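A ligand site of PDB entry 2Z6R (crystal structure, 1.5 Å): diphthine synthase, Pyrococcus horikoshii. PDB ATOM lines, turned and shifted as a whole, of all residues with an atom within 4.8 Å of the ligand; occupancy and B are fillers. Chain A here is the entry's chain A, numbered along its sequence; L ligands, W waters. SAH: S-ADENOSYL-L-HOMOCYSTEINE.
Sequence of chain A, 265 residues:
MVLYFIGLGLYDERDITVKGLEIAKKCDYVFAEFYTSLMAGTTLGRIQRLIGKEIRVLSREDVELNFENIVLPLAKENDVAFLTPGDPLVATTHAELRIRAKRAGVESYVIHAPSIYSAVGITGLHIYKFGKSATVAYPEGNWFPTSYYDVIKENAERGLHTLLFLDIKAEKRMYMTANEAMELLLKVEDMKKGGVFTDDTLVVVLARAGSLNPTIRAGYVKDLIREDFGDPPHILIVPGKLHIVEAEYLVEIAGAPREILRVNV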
ATOM      1  N   LEU A  10      -9.016 -16.788 -13.085  1.00  0.00           N
ATOM      2  CA  LEU A  10      -8.430 -16.550 -14.401  1.00  0.00           C
ATOM      3  C   LEU A  10      -7.351 -17.413 -15.019  1.00  0.00           C
ATOM      4  O   LEU A  10      -7.424 -17.730 -16.209  1.00  0.00           O
ATOM      5  CB  LEU A  10      -7.881 -15.123 -14.432  1.00  0.00           C
ATOM      6  CG  LEU A  10      -8.819 -13.945 -14.195  1.00  0.00           C
ATOM      7  CD1 LEU A  10      -8.000 -12.697 -13.882  1.00  0.00           C
ATOM      8  CD2 LEU A  10      -9.695 -13.738 -15.418  1.00  0.00           C
ATOM      9  N   TYR A  11      -6.357 -17.790 -14.226  1.00  0.00           N
ATOM     10  CA  TYR A  11      -5.212 -18.488 -14.791  1.00  0.00           C
ATOM     11  C   TYR A  11      -4.699 -19.727 -14.078  1.00  0.00           C
ATOM     12  O   TYR A  11      -4.437 -20.756 -14.719  1.00  0.00           O
ATOM     13  CB  TYR A  11      -4.098 -17.440 -14.900  1.00  0.00           C
ATOM     14  CG  TYR A  11      -2.814 -17.886 -15.540  1.00  0.00           C
ATOM     15  CD1 TYR A  11      -2.733 -18.093 -16.920  1.00  0.00           C
ATOM     16  CD2 TYR A  11      -1.670 -18.080 -14.765  1.00  0.00           C
ATOM     17  CE1 TYR A  11      -1.540 -18.491 -17.507  1.00  0.00           C
ATOM     18  CE2 TYR A  11      -0.477 -18.479 -15.353  1.00  0.00           C
ATOM     19  CZ  TYR A  11      -0.421 -18.677 -16.719  1.00  0.00           C
ATOM     20  OH  TYR A  11       0.768 -19.077 -17.290  1.00  0.00           O
ATOM     21  N   THR A  36     -15.912 -24.202 -20.389  1.00  0.00           N
ATOM     22  CA  THR A  36     -16.325 -22.814 -20.607  1.00  0.00           C
ATOM     23  C   THR A  36     -15.145 -21.861 -20.754  1.00  0.00           C
ATOM     24  O   THR A  36     -15.283 -20.762 -21.276  1.00  0.00           O
ATOM     25  CB  THR A  36     -17.253 -22.297 -19.490  1.00  0.00           C
ATOM     26  OG1 THR A  36     -16.608 -22.450 -18.213  1.00  0.00           O
ATOM     27  CG2 THR A  36     -18.572 -23.044 -19.488  1.00  0.00           C
ATOM     28  N   SER A  37     -13.969 -22.276 -20.283  1.00  0.00           N
ATOM     29  CA  SER A  37     -12.776 -21.447 -20.402  1.00  0.00           C
ATOM     30  C   SER A  37     -11.526 -22.282 -20.186  1.00  0.00           C
ATOM     31  O   SER A  37     -11.615 -23.465 -19.847  1.00  0.00           O
ATOM     32  CB  SER A  37     -12.813 -20.295 -19.399  1.00  0.00           C
ATOM     33  OG  SER A  37     -11.800 -19.348 -19.685  1.00  0.00           O
ATOM     34  N   LEU A  38     -10.378 -21.657 -20.398  1.00  0.00           N
ATOM     35  CA  LEU A  38      -9.106 -22.324 -20.233  1.00  0.00           C
ATOM     36  C   LEU A  38      -8.265 -21.671 -19.150  1.00  0.00           C
ATOM     37  O   LEU A  38      -8.024 -20.456 -19.191  1.00  0.00           O
ATOM     38  CB  LEU A  38      -8.320 -22.298 -21.553  1.00  0.00           C
ATOM     39  CG  LEU A  38      -6.864 -22.779 -21.494  1.00  0.00           C
ATOM     40  CD1 LEU A  38      -6.837 -24.291 -21.227  1.00  0.00           C
ATOM     41  CD2 LEU A  38      -6.160 -22.463 -22.809  1.00  0.00           C
ATOM     42  N   PRO A  85     -13.954 -22.438 -14.315  1.00  0.00           N
ATOM     43  CA  PRO A  85     -12.858 -21.472 -14.494  1.00  0.00           C
ATOM     44  C   PRO A  85     -13.498 -20.087 -14.327  1.00  0.00           C
ATOM     45  O   PRO A  85     -14.727 -19.963 -14.445  1.00  0.00           O
ATOM     46  CB  PRO A  85     -12.422 -21.707 -15.943  1.00  0.00           C
ATOM     47  CG  PRO A  85     -12.813 -23.127 -16.216  1.00  0.00           C
ATOM     48  CD  PRO A  85     -14.151 -23.256 -15.529  1.00  0.00           C
ATOM     49  N   GLY A  86     -12.686 -19.075 -14.055  1.00  0.00           N
ATOM     50  CA  GLY A  86     -13.191 -17.709 -13.892  1.00  0.00           C
ATOM     51  C   GLY A  86     -14.304 -17.626 -12.869  1.00  0.00           C
ATOM     52  O   GLY A  86     -14.236 -18.238 -11.813  1.00  0.00           O
ATOM     53  N   ASP A  87     -15.324 -16.822 -13.184  1.00  0.00           N
ATOM     54  CA  ASP A  87     -16.493 -16.685 -12.314  1.00  0.00           C
ATOM     55  C   ASP A  87     -17.522 -17.631 -12.918  1.00  0.00           C
ATOM     56  O   ASP A  87     -17.743 -17.623 -14.125  1.00  0.00           O
ATOM     57  CB  ASP A  87     -17.001 -15.243 -12.328  1.00  0.00           C
ATOM     58  CG  ASP A  87     -18.206 -15.043 -11.436  1.00  0.00           C
ATOM     59  OD1 ASP A  87     -19.277 -15.586 -11.751  1.00  0.00           O
ATOM     60  OD2 ASP A  87     -18.078 -14.338 -10.406  1.00  0.00           O
ATOM     61  N   VAL A  90     -20.458 -15.927 -15.294  1.00  0.00           N
ATOM     62  CA  VAL A  90     -20.098 -14.925 -16.300  1.00  0.00           C
ATOM     63  C   VAL A  90     -19.830 -15.596 -17.639  1.00  0.00           C
ATOM     64  O   VAL A  90     -18.908 -16.390 -17.768  1.00  0.00           O
ATOM     65  CB  VAL A  90     -18.828 -14.143 -15.889  1.00  0.00           C
ATOM     66  CG1 VAL A  90     -18.405 -13.226 -17.027  1.00  0.00           C
ATOM     67  CG2 VAL A  90     -19.097 -13.326 -14.649  1.00  0.00           C
ATOM     68  N   ALA A  91     -20.648 -15.272 -18.639  1.00  0.00           N
ATOM     69  CA  ALA A  91     -20.472 -15.835 -19.968  1.00  0.00           C
ATOM     70  C   ALA A  91     -20.577 -17.361 -19.965  1.00  0.00           C
ATOM     71  O   ALA A  91     -19.834 -18.054 -20.663  1.00  0.00           O
ATOM     72  CB  ALA A  91     -19.135 -15.401 -20.557  1.00  0.00           C
ATOM     73  N   THR A  92     -21.479 -17.866 -19.132  1.00  0.00           N
ATOM     74  CA  THR A  92     -21.860 -19.255 -19.064  1.00  0.00           C
ATOM     75  C   THR A  92     -23.361 -19.287 -18.919  1.00  0.00           C
ATOM     76  O   THR A  92     -24.010 -18.272 -18.758  1.00  0.00           O
ATOM     77  CB  THR A  92     -21.216 -19.920 -17.828  1.00  0.00           C
ATOM     78  OG1 THR A  92     -21.898 -19.491 -16.635  1.00  0.00           O
ATOM     79  CG2 THR A  92     -19.726 -19.571 -17.698  1.00  0.00           C
ATOM     80  N   PRO A 114     -12.082 -14.072  -9.720  1.00  0.00           N
ATOM     81  CA  PRO A 114     -11.782 -13.093 -10.770  1.00  0.00           C
ATOM     82  C   PRO A 114     -12.236 -13.582 -12.146  1.00  0.00           C
ATOM     83  O   PRO A 114     -12.042 -14.739 -12.510  1.00  0.00           O
ATOM     84  CB  PRO A 114     -10.257 -12.907 -10.653  1.00  0.00           C
ATOM     85  CG  PRO A 114      -9.695 -13.967  -9.749  1.00  0.00           C
ATOM     86  CD  PRO A 114     -10.884 -14.451  -8.958  1.00  0.00           C
ATOM     87  N   SER A 115     -12.848 -12.660 -12.884  1.00  0.00           N
ATOM     88  CA  SER A 115     -13.407 -12.921 -14.206  1.00  0.00           C
ATOM     89  C   SER A 115     -12.755 -12.090 -15.295  1.00  0.00           C
ATOM     90  O   SER A 115     -12.343 -10.954 -15.055  1.00  0.00           O
ATOM     91  CB  SER A 115     -14.903 -12.602 -14.164  1.00  0.00           C
ATOM     92  OG  SER A 115     -15.487 -12.646 -15.453  1.00  0.00           O
ATOM     93  N   ILE A 116     -12.673 -12.638 -16.499  1.00  0.00           N
ATOM     94  CA  ILE A 116     -12.077 -11.905 -17.602  1.00  0.00           C
ATOM     95  C   ILE A 116     -12.909 -10.651 -17.921  1.00  0.00           C
ATOM     96  O   ILE A 116     -12.383  -9.653 -18.399  1.00  0.00           O
ATOM     97  CB  ILE A 116     -11.957 -12.791 -18.883  1.00  0.00           C
ATOM     98  CG1 ILE A 116     -11.143 -12.062 -19.944  1.00  0.00           C
ATOM     99  CG2 ILE A 116     -13.337 -13.160 -19.420  1.00  0.00           C
ATOM    100  CD1 ILE A 116      -9.710 -11.777 -19.529  1.00  0.00           C
ATOM    101  N   TYR A 117     -14.204 -10.717 -17.621  1.00  0.00           N
ATOM    102  CA  TYR A 117     -15.115  -9.603 -17.881  1.00  0.00           C
ATOM    103  C   TYR A 117     -14.675  -8.332 -17.144  1.00  0.00           C
ATOM    104  O   TYR A 117     -14.828  -7.227 -17.663  1.00  0.00           O
ATOM    105  CB  TYR A 117     -16.532 -10.014 -17.483  1.00  0.00           C
ATOM    106  CG  TYR A 117     -17.616  -8.982 -17.695  1.00  0.00           C
ATOM    107  CD1 TYR A 117     -17.941  -8.518 -18.981  1.00  0.00           C
ATOM    108  CD2 TYR A 117     -18.361  -8.502 -16.622  1.00  0.00           C
ATOM    109  CE1 TYR A 117     -18.977  -7.600 -19.165  1.00  0.00           C
ATOM    110  CE2 TYR A 117     -19.388  -7.595 -16.805  1.00  0.00           C
ATOM    111  CZ  TYR A 117     -19.694  -7.142 -18.070  1.00  0.00           C
ATOM    112  OH  TYR A 117     -20.718  -6.240 -18.229  1.00  0.00           O
ATOM    113  N   PHE A 165     -15.448 -12.119 -26.369  1.00  0.00           N
ATOM    114  CA  PHE A 165     -15.042 -13.399 -25.811  1.00  0.00           C
ATOM    115  C   PHE A 165     -14.693 -14.225 -27.042  1.00  0.00           C
ATOM    116  O   PHE A 165     -15.356 -14.107 -28.071  1.00  0.00           O
ATOM    117  CB  PHE A 165     -16.215 -14.064 -25.069  1.00  0.00           C
ATOM    118  CG  PHE A 165     -16.653 -13.345 -23.824  1.00  0.00           C
ATOM    119  CD1 PHE A 165     -15.984 -13.547 -22.624  1.00  0.00           C
ATOM    120  CD2 PHE A 165     -17.749 -12.500 -23.844  1.00  0.00           C
ATOM    121  CE1 PHE A 165     -16.409 -12.913 -21.450  1.00  0.00           C
ATOM    122  CE2 PHE A 165     -18.179 -11.853 -22.687  1.00  0.00           C
ATOM    123  CZ  PHE A 165     -17.518 -12.061 -21.483  1.00  0.00           C
ATOM    124  N   LEU A 166     -13.658 -15.051 -26.956  1.00  0.00           N
ATOM    125  CA  LEU A 166     -13.270 -15.867 -28.101  1.00  0.00           C
ATOM    126  C   LEU A 166     -13.673 -17.318 -27.884  1.00  0.00           C
ATOM    127  O   LEU A 166     -13.751 -17.797 -26.756  1.00  0.00           O
ATOM    128  CB  LEU A 166     -11.770 -15.716 -28.359  1.00  0.00           C
ATOM    129  CG  LEU A 166     -11.340 -14.258 -28.541  1.00  0.00           C
ATOM    130  CD1 LEU A 166      -9.867 -14.192 -28.918  1.00  0.00           C
ATOM    131  CD2 LEU A 166     -12.186 -13.591 -29.615  1.00  0.00           C
ATOM    132  N   ASP A 167     -13.936 -18.017 -28.975  1.00  0.00           N
ATOM    133  CA  ASP A 167     -14.396 -19.398 -28.916  1.00  0.00           C
ATOM    134  C   ASP A 167     -13.403 -20.386 -28.304  1.00  0.00           C
ATOM    135  O   ASP A 167     -12.187 -20.163 -28.274  1.00  0.00           O
ATOM    136  CB  ASP A 167     -14.788 -19.875 -30.314  1.00  0.00           C
ATOM    137  CG  ASP A 167     -15.874 -20.934 -30.295  1.00  0.00           C
ATOM    138  OD1 ASP A 167     -16.322 -21.330 -29.202  1.00  0.00           O
ATOM    139  OD2 ASP A 167     -16.276 -21.382 -31.390  1.00  0.00           O
ATOM    140  N   ILE A 168     -13.954 -21.485 -27.811  1.00  0.00           N
ATOM    141  CA  ILE A 168     -13.168 -22.548 -27.205  1.00  0.00           C
ATOM    142  C   ILE A 168     -13.874 -23.873 -27.443  1.00  0.00           C
ATOM    143  O   ILE A 168     -15.085 -23.979 -27.272  1.00  0.00           O
ATOM    144  CB  ILE A 168     -12.982 -22.336 -25.678  1.00  0.00           C
ATOM    145  CG1 ILE A 168     -12.396 -23.604 -25.047  1.00  0.00           C
ATOM    146  CG2 ILE A 168     -14.315 -21.964 -25.031  1.00  0.00           C
ATOM    147  CD1 ILE A 168     -12.070 -23.482 -23.566  1.00  0.00           C
ATOM    148  N   LEU A 206      -5.721  -8.960 -24.911  1.00  0.00           N
ATOM    149  CA  LEU A 206      -5.334  -9.351 -23.559  1.00  0.00           C
ATOM    150  C   LEU A 206      -5.227 -10.870 -23.560  1.00  0.00           C
ATOM    151  O   LEU A 206      -6.208 -11.575 -23.837  1.00  0.00           O
ATOM    152  CB  LEU A 206      -6.369  -8.879 -22.525  1.00  0.00           C
ATOM    153  CG  LEU A 206      -6.107  -9.300 -21.071  1.00  0.00           C
ATOM    154  CD1 LEU A 206      -4.738  -8.809 -20.608  1.00  0.00           C
ATOM    155  CD2 LEU A 206      -7.207  -8.735 -20.178  1.00  0.00           C
ATOM    156  N   ALA A 207      -4.032 -11.374 -23.283  1.00  0.00           N
ATOM    157  CA  ALA A 207      -3.795 -12.807 -23.274  1.00  0.00           C
ATOM    158  C   ALA A 207      -3.285 -13.282 -21.918  1.00  0.00           C
ATOM    159  O   ALA A 207      -2.369 -12.710 -21.342  1.00  0.00           O
ATOM    160  CB  ALA A 207      -2.793 -13.182 -24.359  1.00  0.00           C
ATOM    161  N   ARG A 208      -3.907 -14.355 -21.419  1.00  0.00           N
ATOM    162  CA  ARG A 208      -3.530 -14.950 -20.147  1.00  0.00           C
ATOM    163  C   ARG A 208      -3.648 -14.005 -18.954  1.00  0.00           C
ATOM    164  O   ARG A 208      -2.738 -13.876 -18.131  1.00  0.00           O
ATOM    165  CB  ARG A 208      -2.095 -15.512 -20.242  1.00  0.00           C
ATOM    166  CG  ARG A 208      -1.920 -16.551 -21.361  1.00  0.00           C
ATOM    167  CD  ARG A 208      -0.469 -17.028 -21.456  1.00  0.00           C
ATOM    168  NE  ARG A 208       0.449 -15.905 -21.491  1.00  0.00           N
ATOM    169  CZ  ARG A 208       0.592 -15.069 -22.525  1.00  0.00           C
ATOM    170  NH1 ARG A 208      -0.128 -15.237 -23.634  1.00  0.00           N
ATOM    171  NH2 ARG A 208       1.423 -14.043 -22.426  1.00  0.00           N
ATOM    172  N   ALA A 209      -4.785 -13.331 -18.862  1.00  0.00           N
ATOM    173  CA  ALA A 209      -5.041 -12.447 -17.731  1.00  0.00           C
ATOM    174  C   ALA A 209      -4.974 -13.347 -16.502  1.00  0.00           C
ATOM    175  O   ALA A 209      -5.303 -14.532 -16.582  1.00  0.00           O
ATOM    176  CB  ALA A 209      -6.413 -11.812 -17.848  1.00  0.00           C
ATOM    177  N   PRO A 233      -5.498 -18.536 -23.024  1.00  0.00           N
ATOM    178  CA  PRO A 233      -6.605 -17.872 -23.724  1.00  0.00           C
ATOM    179  C   PRO A 233      -6.349 -16.401 -24.057  1.00  0.00           C
ATOM    180  O   PRO A 233      -5.532 -15.733 -23.427  1.00  0.00           O
ATOM    181  CB  PRO A 233      -7.757 -18.042 -22.750  1.00  0.00           C
ATOM    182  CG  PRO A 233      -7.077 -17.893 -21.438  1.00  0.00           C
ATOM    183  CD  PRO A 233      -5.814 -18.724 -21.597  1.00  0.00           C
ATOM    184  N   HIS A 234      -7.077 -15.934 -25.067  1.00  0.00           N
ATOM    185  CA  HIS A 234      -7.002 -14.543 -25.521  1.00  0.00           C
ATOM    186  C   HIS A 234      -8.407 -13.964 -25.549  1.00  0.00           C
ATOM    187  O   HIS A 234      -9.389 -14.686 -25.673  1.00  0.00           O
ATOM    188  CB  HIS A 234      -6.517 -14.430 -26.968  1.00  0.00           C
ATOM    189  CG  HIS A 234      -5.139 -14.921 -27.221  1.00  0.00           C
ATOM    190  ND1 HIS A 234      -4.575 -14.906 -28.486  1.00  0.00           N
ATOM    191  CD2 HIS A 234      -4.188 -15.440 -26.403  1.00  0.00           C
ATOM    192  CE1 HIS A 234      -3.351 -15.391 -28.431  1.00  0.00           C
ATOM    193  NE2 HIS A 234      -3.089 -15.726 -27.182  1.00  0.00           N
ATOM    194  N   ILE A 235      -8.468 -12.646 -25.445  1.00  0.00           N
ATOM    195  CA  ILE A 235      -9.721 -11.927 -25.601  1.00  0.00           C
ATOM    196  C   ILE A 235      -9.367 -10.749 -26.498  1.00  0.00           C
ATOM    197  O   ILE A 235      -8.233 -10.246 -26.452  1.00  0.00           O
ATOM    198  CB  ILE A 235     -10.301 -11.415 -24.256  1.00  0.00           C
ATOM    199  CG1 ILE A 235     -11.812 -11.228 -24.400  1.00  0.00           C
ATOM    200  CG2 ILE A 235      -9.631 -10.125 -23.827  1.00  0.00           C
ATOM    201  CD1 ILE A 235     -12.589 -11.495 -23.124  1.00  0.00           C
HETATM  202  N   SAH L   1     -16.747 -17.446 -16.689  1.00  0.00           N
HETATM  203  CA  SAH L   1     -15.463 -17.026 -17.396  1.00  0.00           C
HETATM  204  CB  SAH L   1     -15.585 -16.701 -18.855  1.00  0.00           C
HETATM  205  CG  SAH L   1     -16.139 -17.768 -19.790  1.00  0.00           C
HETATM  206  SD  SAH L   1     -15.926 -17.194 -21.521  1.00  0.00           S
HETATM  207  C   SAH L   1     -14.885 -15.785 -16.600  1.00  0.00           C
HETATM  208  O   SAH L   1     -15.508 -15.350 -15.619  1.00  0.00           O
HETATM  209  OXT SAH L   1     -13.769 -15.310 -17.034  1.00  0.00           O
HETATM  210  C5' SAH L   1     -14.354 -17.880 -21.866  1.00  0.00           C
HETATM  211  C4' SAH L   1     -13.514 -16.934 -22.824  1.00  0.00           C
HETATM  212  O4' SAH L   1     -13.137 -15.757 -22.061  1.00  0.00           O
HETATM  213  C3' SAH L   1     -12.244 -17.519 -23.331  1.00  0.00           C
HETATM  214  O3' SAH L   1     -12.462 -18.322 -24.488  1.00  0.00           O
HETATM  215  C2' SAH L   1     -11.397 -16.239 -23.554  1.00  0.00           C
HETATM  216  O2' SAH L   1     -11.722 -15.600 -24.793  1.00  0.00           O
HETATM  217  C1' SAH L   1     -11.715 -15.379 -22.319  1.00  0.00           C
HETATM  218  N9  SAH L   1     -10.969 -15.625 -21.214  1.00  0.00           N
HETATM  219  C8  SAH L   1     -11.184 -16.320 -20.039  1.00  0.00           C
HETATM  220  N7  SAH L   1     -10.187 -16.310 -19.198  1.00  0.00           N
HETATM  221  C5  SAH L   1      -9.191 -15.536 -19.834  1.00  0.00           C
HETATM  222  C6  SAH L   1      -7.871 -15.149 -19.408  1.00  0.00           C
HETATM  223  N6  SAH L   1      -7.328 -15.508 -18.229  1.00  0.00           N
HETATM  224  N1  SAH L   1      -7.184 -14.377 -20.312  1.00  0.00           N
HETATM  225  C2  SAH L   1      -7.691 -13.990 -21.510  1.00  0.00           C
HETATM  226  N3  SAH L   1      -8.940 -14.339 -21.954  1.00  0.00           N
HETATM  227  C4  SAH L   1      -9.640 -15.105 -21.064  1.00  0.00           C
HETATM  228  O   HOH W   1     -16.049 -20.185 -16.918  1.00  0.00           O
HETATM  229  O   HOH W   2     -10.530 -19.753 -25.930  1.00  0.00           O
HETATM  230  O   HOH W   3     -11.183 -16.812 -16.610  1.00  0.00           O
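Water W2 lies within hydrogen-bond range of O3' of the ligand and O of Asp 167. Water W1 lies within hydrogen-bond range of the side-chain hydroxyl of Thr 36 (2.7 Å), the backbone carbonyl oxygen of Pro 85 (2.8 Å) and a nitrogen (N) of the ligand (2.8 Å).
The backbone NH (N) of Tyr 117 lies close to the side-chain hydroxyl (OG) of Ser 115 (3.2 Å). The backbone NH (N) of Arg 208 is in hydrogen-bond range of the backbone carbonyl oxygen (O) of Pro 233 (2.9 Å). The backbone NH of Ile 235 is in hydrogen-bond range of the backbone carbonyl oxygen of Leu 206 (3.0 Å).
O of Thr 36 lies close to SD of the ligand, 3.6 Å away. Residues that only touch the ligand: Pro 85 (3.9 Å), Gly 86 (3.7 Å), Ala 91 (3.8 Å), Thr 92 (3.8 Å), Phe 165 (3.6 Å), Leu 206 (3.7 Å), Pro 233 (3.4 Å) and Ile 235 (3.9 Å). Hydrophobic or aromatic side chains within 4 Å of the ligand: Leu 10, Val 90, Ala 91, Ile 116, Phe 165, Leu 166, Ala 209, Pro 233 and Ile 235. Within 4 Å of the ligand: Leu 10, Thr 36, Ser 37, Pro 85, Gly 86, Asp 87, Val 90, Ala 91, Thr 92, Ser 115, Ile 116, Phe 165, Leu 166, Leu 206, Arg 208, Ala 209, Pro 233, His 234 and Ile 235. The nearest printed residue that does not touch the ligand is Ile 168 (4.1 Å).
A nitrogen (N) of the ligand sits at hydrogen-bond distance from the backbone carbonyl oxygen (O) of Val 90 (2.6 Å). An oxygen (O2') of the ligand is in hydrogen-bond range of the backbone carbonyl oxygen (O) of His 234. O2' of the ligand sits at hydrogen-bond distance from N of Leu 166 (3.0 Å). An oxygen (O3') of the ligand is in hydrogen-bond range of the backbone carbonyl oxygen (O) of Leu 166, 2.7 Å away. OG of Ser 115 sits at hydrogen-bond distance from O of the ligand. The backbone NH of Asp 87 is in hydrogen-bond range of an oxygen (O) of the ligand (2.9 Å). The backbone carbonyl oxygen (O) of Asp 87 lies within hydrogen-bond range of a nitrogen (N) of the ligand, 2.8 Å away. The backbone NH (N) of Ala 209 lies within hydrogen-bond range of a nitrogen (N1) of the ligand (3.0 Å). A nitrogen (N6) of the ligand lies within hydrogen-bond range of the backbone carbonyl oxygen (O) of Ala 209 (2.8 Å). The backbone NH of Ile 116 lies within hydrogen-bond range of an oxygen (OXT) of the ligand, at 2.9 Å. A nitrogen (N6) of the ligand is in hydrogen-bond range of the backbone carbonyl oxygen (O) of Leu 10, at 3.0 Å. OG of Ser 37 sits close to N7 of the ligand, at 3.5 Å. N1 of the ligand sits at hydrogen-bond distance from N of Arg 208 (3.5 Å).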
